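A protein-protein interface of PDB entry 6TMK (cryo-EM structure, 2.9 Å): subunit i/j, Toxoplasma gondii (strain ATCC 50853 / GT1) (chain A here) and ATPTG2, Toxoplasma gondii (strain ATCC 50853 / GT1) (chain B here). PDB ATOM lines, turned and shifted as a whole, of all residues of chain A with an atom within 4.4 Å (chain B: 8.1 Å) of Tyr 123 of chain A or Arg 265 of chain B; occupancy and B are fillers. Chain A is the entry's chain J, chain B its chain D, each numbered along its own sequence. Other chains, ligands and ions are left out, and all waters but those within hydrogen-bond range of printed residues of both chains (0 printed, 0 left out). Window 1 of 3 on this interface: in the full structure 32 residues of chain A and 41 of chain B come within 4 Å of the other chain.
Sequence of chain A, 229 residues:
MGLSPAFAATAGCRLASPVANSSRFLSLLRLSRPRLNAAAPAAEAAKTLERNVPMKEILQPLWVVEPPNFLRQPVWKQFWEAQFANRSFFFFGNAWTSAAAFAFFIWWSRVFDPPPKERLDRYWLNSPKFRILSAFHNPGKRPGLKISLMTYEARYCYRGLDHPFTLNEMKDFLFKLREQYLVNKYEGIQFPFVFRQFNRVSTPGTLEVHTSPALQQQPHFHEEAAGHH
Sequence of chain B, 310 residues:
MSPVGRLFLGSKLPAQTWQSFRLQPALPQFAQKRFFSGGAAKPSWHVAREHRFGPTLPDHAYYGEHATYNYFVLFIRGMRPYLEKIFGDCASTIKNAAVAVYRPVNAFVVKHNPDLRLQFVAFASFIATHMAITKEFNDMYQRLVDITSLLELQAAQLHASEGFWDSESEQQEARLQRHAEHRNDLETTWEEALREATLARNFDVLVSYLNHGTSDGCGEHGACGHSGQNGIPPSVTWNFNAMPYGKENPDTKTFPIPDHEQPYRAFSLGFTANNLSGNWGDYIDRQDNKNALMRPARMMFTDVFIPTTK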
ATOM      1  N   LEU A 120       6.882   7.282   9.187  1.00  0.00           N
ATOM      2  CA  LEU A 120       7.179   8.377  10.106  1.00  0.00           C
ATOM      3  C   LEU A 120       8.205   7.974  11.160  1.00  0.00           C
ATOM      4  O   LEU A 120       9.040   8.791  11.566  1.00  0.00           O
ATOM      5  CB  LEU A 120       5.914   8.848  10.812  1.00  0.00           C
ATOM      6  CG  LEU A 120       4.911   9.709  10.067  1.00  0.00           C
ATOM      7  CD1 LEU A 120       3.667   9.801  10.903  1.00  0.00           C
ATOM      8  CD2 LEU A 120       5.465  11.069   9.782  1.00  0.00           C
ATOM      9  N   ASP A 121       8.161   6.726  11.614  1.00  0.00           N
ATOM     10  CA  ASP A 121       9.083   6.225  12.622  1.00  0.00           C
ATOM     11  C   ASP A 121      10.436   5.842  12.052  1.00  0.00           C
ATOM     12  O   ASP A 121      11.252   5.258  12.769  1.00  0.00           O
ATOM     13  CB  ASP A 121       8.471   5.027  13.343  1.00  0.00           C
ATOM     14  CG  ASP A 121       8.289   3.839  12.438  1.00  0.00           C
ATOM     15  OD1 ASP A 121       7.603   3.977  11.404  1.00  0.00           O
ATOM     16  OD2 ASP A 121       8.837   2.762  12.746  1.00  0.00           O
ATOM     17  N   ARG A 122      10.688   6.151  10.784  1.00  0.00           N
ATOM     18  CA  ARG A 122      12.006   5.944  10.207  1.00  0.00           C
ATOM     19  C   ARG A 122      12.957   7.066  10.604  1.00  0.00           C
ATOM     20  O   ARG A 122      14.100   6.811  10.996  1.00  0.00           O
ATOM     21  CB  ARG A 122      11.898   5.843   8.686  1.00  0.00           C
ATOM     22  CG  ARG A 122      13.060   5.155   8.025  1.00  0.00           C
ATOM     23  CD  ARG A 122      12.954   3.654   8.116  1.00  0.00           C
ATOM     24  NE  ARG A 122      14.188   2.989   7.718  1.00  0.00           N
ATOM     25  CZ  ARG A 122      14.524   2.707   6.468  1.00  0.00           C
ATOM     26  NH1 ARG A 122      13.726   3.023   5.464  1.00  0.00           N
ATOM     27  NH2 ARG A 122      15.667   2.099   6.225  1.00  0.00           N
ATOM     28  N   TYR A 123      12.510   8.303  10.494  1.00  0.00           N
ATOM     29  CA  TYR A 123      13.304   9.453  10.903  1.00  0.00           C
ATOM     30  C   TYR A 123      12.554  10.438  11.785  1.00  0.00           C
ATOM     31  O   TYR A 123      13.135  10.951  12.741  1.00  0.00           O
ATOM     32  CB  TYR A 123      13.826  10.169   9.658  1.00  0.00           C
ATOM     33  CG  TYR A 123      14.896  11.189   9.922  1.00  0.00           C
ATOM     34  CD1 TYR A 123      16.223  10.873   9.736  1.00  0.00           C
ATOM     35  CD2 TYR A 123      14.583  12.470  10.338  1.00  0.00           C
ATOM     36  CE1 TYR A 123      17.205  11.791   9.963  1.00  0.00           C
ATOM     37  CE2 TYR A 123      15.559  13.390  10.573  1.00  0.00           C
ATOM     38  CZ  TYR A 123      16.870  13.052  10.384  1.00  0.00           C
ATOM     39  OH  TYR A 123      17.847  13.983  10.619  1.00  0.00           O
ATOM     40  N   TRP A 124      11.275  10.695  11.512  1.00  0.00           N
ATOM     41  CA  TRP A 124      10.650  11.916  12.010  1.00  0.00           C
ATOM     42  C   TRP A 124      10.391  11.841  13.505  1.00  0.00           C
ATOM     43  O   TRP A 124      10.565  12.835  14.219  1.00  0.00           O
ATOM     44  CB  TRP A 124       9.345  12.190  11.270  1.00  0.00           C
ATOM     45  CG  TRP A 124       8.575  13.346  11.814  1.00  0.00           C
ATOM     46  CD1 TRP A 124       7.336  13.307  12.363  1.00  0.00           C
ATOM     47  CD2 TRP A 124       8.991  14.714  11.871  1.00  0.00           C
ATOM     48  NE1 TRP A 124       6.952  14.552  12.760  1.00  0.00           N
ATOM     49  CE2 TRP A 124       7.950  15.437  12.466  1.00  0.00           C
ATOM     50  CE3 TRP A 124      10.140  15.396  11.478  1.00  0.00           C
ATOM     51  CZ2 TRP A 124       8.022  16.796  12.680  1.00  0.00           C
ATOM     52  CZ3 TRP A 124      10.203  16.745  11.688  1.00  0.00           C
ATOM     53  CH2 TRP A 124       9.156  17.432  12.283  1.00  0.00           C
ATOM     54  N   LEU A 125       9.978  10.682  14.005  1.00  0.00           N
ATOM     55  CA  LEU A 125       9.650  10.565  15.414  1.00  0.00           C
ATOM     56  C   LEU A 125      10.877  10.520  16.310  1.00  0.00           C
ATOM     57  O   LEU A 125      10.729  10.524  17.535  1.00  0.00           O
ATOM     58  CB  LEU A 125       8.795   9.319  15.631  1.00  0.00           C
ATOM     59  CG  LEU A 125       7.529   9.262  14.780  1.00  0.00           C
ATOM     60  CD1 LEU A 125       6.789   7.982  15.012  1.00  0.00           C
ATOM     61  CD2 LEU A 125       6.634  10.430  15.083  1.00  0.00           C
ATOM     62  N   ASN A 126      12.075  10.493  15.735  1.00  0.00           N
ATOM     63  CA  ASN A 126      13.323  10.557  16.481  1.00  0.00           C
ATOM     64  C   ASN A 126      14.114  11.794  16.080  1.00  0.00           C
ATOM     65  O   ASN A 126      15.342  11.785  16.069  1.00  0.00           O
ATOM     66  CB  ASN A 126      14.155   9.295  16.276  1.00  0.00           C
ATOM     67  CG  ASN A 126      13.372   8.041  16.517  1.00  0.00           C
ATOM     68  OD1 ASN A 126      13.023   7.321  15.585  1.00  0.00           O
ATOM     69  ND2 ASN A 126      13.100   7.762  17.775  1.00  0.00           N
ATOM     70  N   SER A 127      13.420  12.853  15.783  1.00  0.00           N
ATOM     71  CA  SER A 127      13.994  14.052  15.208  1.00  0.00           C
ATOM     72  C   SER A 127      14.042  15.172  16.235  1.00  0.00           C
ATOM     73  O   SER A 127      13.127  15.299  17.057  1.00  0.00           O
ATOM     74  CB  SER A 127      13.192  14.511  13.989  1.00  0.00           C
ATOM     75  OG  SER A 127      13.706  15.697  13.441  1.00  0.00           O
ATOM     76  N   LYS B 247      21.012  -2.027  23.311  1.00  0.00           N
ATOM     77  CA  LYS B 247      21.225  -2.101  21.875  1.00  0.00           C
ATOM     78  C   LYS B 247      22.069  -3.313  21.508  1.00  0.00           C
ATOM     79  O   LYS B 247      21.769  -4.018  20.539  1.00  0.00           O
ATOM     80  CB  LYS B 247      21.893  -0.816  21.395  1.00  0.00           C
ATOM     81  CG  LYS B 247      21.826  -0.606  19.907  1.00  0.00           C
ATOM     82  CD  LYS B 247      22.956   0.272  19.418  1.00  0.00           C
ATOM     83  CE  LYS B 247      22.561   1.049  18.177  1.00  0.00           C
ATOM     84  NZ  LYS B 247      21.815   0.217  17.194  1.00  0.00           N
ATOM     85  N   GLN B 262      14.666  -0.960  10.282  1.00  0.00           N
ATOM     86  CA  GLN B 262      15.334  -0.313  11.400  1.00  0.00           C
ATOM     87  C   GLN B 262      15.289   1.207  11.232  1.00  0.00           C
ATOM     88  O   GLN B 262      15.349   1.713  10.108  1.00  0.00           O
ATOM     89  CB  GLN B 262      16.780  -0.778  11.509  1.00  0.00           C
ATOM     90  CG  GLN B 262      16.915  -2.223  11.899  1.00  0.00           C
ATOM     91  CD  GLN B 262      18.194  -2.499  12.634  1.00  0.00           C
ATOM     92  OE1 GLN B 262      19.233  -2.760  12.028  1.00  0.00           O
ATOM     93  NE2 GLN B 262      18.137  -2.416  13.952  1.00  0.00           N
ATOM     94  N   PRO B 263      15.185   1.978  12.311  1.00  0.00           N
ATOM     95  CA  PRO B 263      15.063   3.429  12.180  1.00  0.00           C
ATOM     96  C   PRO B 263      16.400   4.150  12.064  1.00  0.00           C
ATOM     97  O   PRO B 263      17.449   3.658  12.476  1.00  0.00           O
ATOM     98  CB  PRO B 263      14.341   3.819  13.474  1.00  0.00           C
ATOM     99  CG  PRO B 263      14.825   2.863  14.445  1.00  0.00           C
ATOM    100  CD  PRO B 263      15.049   1.562  13.717  1.00  0.00           C
ATOM    101  N   TYR B 264      16.329   5.353  11.505  1.00  0.00           N
ATOM    102  CA  TYR B 264      17.517   6.154  11.261  1.00  0.00           C
ATOM    103  C   TYR B 264      17.777   7.133  12.392  1.00  0.00           C
ATOM    104  O   TYR B 264      16.854   7.659  13.018  1.00  0.00           O
ATOM    105  CB  TYR B 264      17.377   6.964   9.973  1.00  0.00           C
ATOM    106  CG  TYR B 264      17.433   6.188   8.687  1.00  0.00           C
ATOM    107  CD1 TYR B 264      18.406   5.237   8.460  1.00  0.00           C
ATOM    108  CD2 TYR B 264      16.516   6.436   7.683  1.00  0.00           C
ATOM    109  CE1 TYR B 264      18.452   4.541   7.281  1.00  0.00           C
ATOM    110  CE2 TYR B 264      16.553   5.750   6.503  1.00  0.00           C
ATOM    111  CZ  TYR B 264      17.525   4.802   6.303  1.00  0.00           C
ATOM    112  OH  TYR B 264      17.565   4.110   5.119  1.00  0.00           O
ATOM    113  N   ARG B 265      19.056   7.377  12.639  1.00  0.00           N
ATOM    114  CA  ARG B 265      19.476   8.418  13.558  1.00  0.00           C
ATOM    115  C   ARG B 265      19.462   9.774  12.866  1.00  0.00           C
ATOM    116  O   ARG B 265      19.691   9.885  11.658  1.00  0.00           O
ATOM    117  CB  ARG B 265      20.871   8.118  14.091  1.00  0.00           C
ATOM    118  CG  ARG B 265      21.337   9.024  15.177  1.00  0.00           C
ATOM    119  CD  ARG B 265      22.667   8.579  15.692  1.00  0.00           C
ATOM    120  NE  ARG B 265      23.241   9.522  16.636  1.00  0.00           N
ATOM    121  CZ  ARG B 265      24.108  10.475  16.323  1.00  0.00           C
ATOM    122  NH1 ARG B 265      24.519  10.640  15.078  1.00  0.00           N
ATOM    123  NH2 ARG B 265      24.561  11.272  17.266  1.00  0.00           N
ATOM    124  N   ALA B 266      19.195  10.812  13.644  1.00  0.00           N
ATOM    125  CA  ALA B 266      19.094  12.151  13.088  1.00  0.00           C
ATOM    126  C   ALA B 266      20.441  12.615  12.554  1.00  0.00           C
ATOM    127  O   ALA B 266      21.501  12.231  13.056  1.00  0.00           O
ATOM    128  CB  ALA B 266      18.582  13.137  14.129  1.00  0.00           C
ATOM    129  N   PHE B 267      20.392  13.449  11.522  1.00  0.00           N
ATOM    130  CA  PHE B 267      21.583  13.956  10.865  1.00  0.00           C
ATOM    131  C   PHE B 267      21.638  15.468  10.990  1.00  0.00           C
ATOM    132  O   PHE B 267      20.669  16.160  10.664  1.00  0.00           O
ATOM    133  CB  PHE B 267      21.612  13.557   9.395  1.00  0.00           C
ATOM    134  CG  PHE B 267      22.941  13.752   8.753  1.00  0.00           C
ATOM    135  CD1 PHE B 267      23.959  12.852   8.969  1.00  0.00           C
ATOM    136  CD2 PHE B 267      23.177  14.842   7.944  1.00  0.00           C
ATOM    137  CE1 PHE B 267      25.182  13.031   8.385  1.00  0.00           C
ATOM    138  CE2 PHE B 267      24.398  15.024   7.358  1.00  0.00           C
ATOM    139  CZ  PHE B 267      25.404  14.118   7.578  1.00  0.00           C
ATOM    140  N   SER B 268      22.780  15.973  11.446  1.00  0.00           N
ATOM    141  CA  SER B 268      23.059  17.400  11.469  1.00  0.00           C
ATOM    142  C   SER B 268      24.516  17.605  11.100  1.00  0.00           C
ATOM    143  O   SER B 268      25.406  17.054  11.754  1.00  0.00           O
ATOM    144  CB  SER B 268      22.768  18.005  12.842  1.00  0.00           C
ATOM    145  OG  SER B 268      23.289  19.316  12.941  1.00  0.00           O
ATOM    146  N   ASN B 274      27.408  20.086  14.381  1.00  0.00           N
ATOM    147  CA  ASN B 274      27.080  18.773  13.856  1.00  0.00           C
ATOM    148  C   ASN B 274      26.619  17.900  15.015  1.00  0.00           C
ATOM    149  O   ASN B 274      26.627  18.316  16.175  1.00  0.00           O
ATOM    150  CB  ASN B 274      28.268  18.146  13.117  1.00  0.00           C
ATOM    151  CG  ASN B 274      29.469  17.947  14.002  1.00  0.00           C
ATOM    152  OD1 ASN B 274      29.526  17.011  14.794  1.00  0.00           O
ATOM    153  ND2 ASN B 274      30.447  18.822  13.862  1.00  0.00           N
ATOM    154  N   ASN B 275      26.219  16.673  14.688  1.00  0.00           N
ATOM    155  CA  ASN B 275      25.782  15.693  15.675  1.00  0.00           C
ATOM    156  C   ASN B 275      26.510  14.372  15.480  1.00  0.00           C
ATOM    157  O   ASN B 275      25.990  13.310  15.825  1.00  0.00           O
ATOM    158  CB  ASN B 275      24.269  15.496  15.621  1.00  0.00           C
ATOM    159  CG  ASN B 275      23.813  14.777  14.380  1.00  0.00           C
ATOM    160  OD1 ASN B 275      24.264  15.063  13.275  1.00  0.00           O
ATOM    161  ND2 ASN B 275      22.898  13.841  14.555  1.00  0.00           N
ATOM    162  N   LEU B 276      27.718  14.428  14.931  1.00  0.00           N
ATOM    163  CA  LEU B 276      28.500  13.243  14.631  1.00  0.00           C
ATOM    164  C   LEU B 276      29.775  13.149  15.451  1.00  0.00           C
ATOM    165  O   LEU B 276      30.389  12.077  15.488  1.00  0.00           O
ATOM    166  CB  LEU B 276      28.863  13.224  13.143  1.00  0.00           C
ATOM    167  CG  LEU B 276      27.776  13.692  12.183  1.00  0.00           C
ATOM    168  CD1 LEU B 276      28.349  13.770  10.807  1.00  0.00           C
ATOM    169  CD2 LEU B 276      26.567  12.787  12.211  1.00  0.00           C
ATOM    170  N   SER B 277      30.191  14.231  16.097  1.00  0.00           N
ATOM    171  CA  SER B 277      31.336  14.207  16.994  1.00  0.00           C
ATOM    172  C   SER B 277      31.018  13.588  18.344  1.00  0.00           C
ATOM    173  O   SER B 277      31.900  13.543  19.206  1.00  0.00           O
ATOM    174  CB  SER B 277      31.853  15.627  17.213  1.00  0.00           C
ATOM    175  OG  SER B 277      30.837  16.458  17.741  1.00  0.00           O
ATOM    176  N   GLY B 278      29.799  13.106  18.551  1.00  0.00           N
ATOM    177  CA  GLY B 278      29.442  12.551  19.840  1.00  0.00           C
ATOM    178  C   GLY B 278      28.224  11.666  19.754  1.00  0.00           C
ATOM    179  O   GLY B 278      27.566  11.557  18.717  1.00  0.00           O
ATOM    180  N   ASN B 279      27.940  11.023  20.881  1.00  0.00           N
ATOM    181  CA  ASN B 279      26.786  10.149  21.026  1.00  0.00           C
ATOM    182  C   ASN B 279      26.141  10.415  22.374  1.00  0.00           C
ATOM    183  O   ASN B 279      26.805  10.325  23.410  1.00  0.00           O
ATOM    184  CB  ASN B 279      27.191   8.683  20.900  1.00  0.00           C
ATOM    185  CG  ASN B 279      26.011   7.764  20.765  1.00  0.00           C
ATOM    186  OD1 ASN B 279      25.066   8.049  20.034  1.00  0.00           O
ATOM    187  ND2 ASN B 279      26.057   6.646  21.468  1.00  0.00           N
ATOM    188  N   TRP B 280      24.856  10.752  22.355  1.00  0.00           N
ATOM    189  CA  TRP B 280      24.110  11.047  23.565  1.00  0.00           C
ATOM    190  C   TRP B 280      23.478   9.811  24.178  1.00  0.00           C
ATOM    191  O   TRP B 280      23.082   9.846  25.347  1.00  0.00           O
ATOM    192  CB  TRP B 280      23.009  12.061  23.259  1.00  0.00           C
ATOM    193  CG  TRP B 280      23.493  13.442  23.005  1.00  0.00           C
ATOM    194  CD1 TRP B 280      23.410  14.500  23.843  1.00  0.00           C
ATOM    195  CD2 TRP B 280      24.126  13.919  21.820  1.00  0.00           C
ATOM    196  NE1 TRP B 280      23.952  15.609  23.261  1.00  0.00           N
ATOM    197  CE2 TRP B 280      24.402  15.278  22.015  1.00  0.00           C
ATOM    198  CE3 TRP B 280      24.493  13.327  20.614  1.00  0.00           C
ATOM    199  CZ2 TRP B 280      25.022  16.055  21.050  1.00  0.00           C
ATOM    200  CZ3 TRP B 280      25.108  14.099  19.665  1.00  0.00           C
ATOM    201  CH2 TRP B 280      25.368  15.445  19.886  1.00  0.00           C
ATOM    202  N   GLY B 281      23.365   8.741  23.416  1.00  0.00           N
ATOM    203  CA  GLY B 281      22.774   7.517  23.889  1.00  0.00           C
ATOM    204  C   GLY B 281      21.282   7.465  23.665  1.00  0.00           C
ATOM    205  O   GLY B 281      20.679   8.301  22.989  1.00  0.00           O
ATOM    206  N   ASN B 289      28.172  13.136  25.588  1.00  0.00           N
ATOM    207  CA  ASN B 289      28.538  13.395  24.200  1.00  0.00           C
ATOM    208  C   ASN B 289      30.002  13.793  24.074  1.00  0.00           C
ATOM    209  O   ASN B 289      30.678  13.398  23.118  1.00  0.00           O
ATOM    210  CB  ASN B 289      27.628  14.463  23.604  1.00  0.00           C
ATOM    211  CG  ASN B 289      27.522  15.692  24.474  1.00  0.00           C
ATOM    212  OD1 ASN B 289      27.404  15.598  25.692  1.00  0.00           O
ATOM    213  ND2 ASN B 289      27.570  16.856  23.851  1.00  0.00           N
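Among the printed residues, merely in contact across the chains: Asp 121 of chain A with Pro 263 of chain B (3.5 Å), Arg 122 of chain A with Pro 263 of chain B (3.7 Å), Tyr 123 of chain A with Arg 265 of chain B (3.6 Å) and Tyr 123 of chain A with Ala 266 of chain B (3.3 Å).
The backbone carbonyl oxygen (O) of Ala 266 of chain B is in hydrogen-bond range of the side-chain amide nitrogen (ND2) of Asn 275 of chain B.
The guanidinium group (NH2) of Arg 265 of chain B is in hydrogen-bond range of the backbone carbonyl oxygen (O) of Asn 275 of chain B (2.9 Å).
The guanidinium group (NH2) of Arg 265 of chain B lies within hydrogen-bond range of the backbone carbonyl oxygen (O) of Gly 278 of chain B (3.3 Å).
The backbone carbonyl oxygen (O) of Arg 122 of chain A sits at hydrogen-bond distance from the backbone NH (N) of Tyr 264 of chain B, at 2.7 Å.
OH of Tyr 123 of chain A is in hydrogen-bond range of N of Phe 267 of chain B (2.8 Å).
The backbone carbonyl oxygen (O) of Gln 262 of chain B lies within hydrogen-bond range of the guanidinium group (NE) of Arg 122 of chain A.
Of the printed residues of chain B, Tyr 123 of chain A touches Arg 265 (3.6 Å), Ala 266 (3.3 Å) and Phe 267 (2.8 Å).
Arg 265 of chain B touches just one residue of chain A: Tyr 123.
Printed residues of chain A within 4 Å of Gln 262 of chain B: Arg 122 (2.9 Å).
Of the printed residues of chain A, Pro 263 of chain B touches Asp 121 (3.5 Å) and Arg 122 (3.7 Å).
Printed residues of chain A within 4 Å of Ala 266 of chain B: Tyr 123 (3.3 Å).
The nearest residue of chain B that does not touch Tyr 123 of chain A is Tyr 264 of chain B (4.1 Å).
The nearest printed residue of chain A that does not touch Arg 265 of chain B is Arg 122 of chain A (5.3 Å).
Of the 8 printed residues of chain A, 3 touch a printed residue of chain B.
Of the 17 printed residues of chain B, 6 touch a printed residue of chain A.
Hydrophobic or aromatic side chains of chain B within 4 Å of the printed part of chain A: Pro 263, Tyr 264, Ala 266 and Phe 267.
Among the printed residues, 7 pairs touch across the chains.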
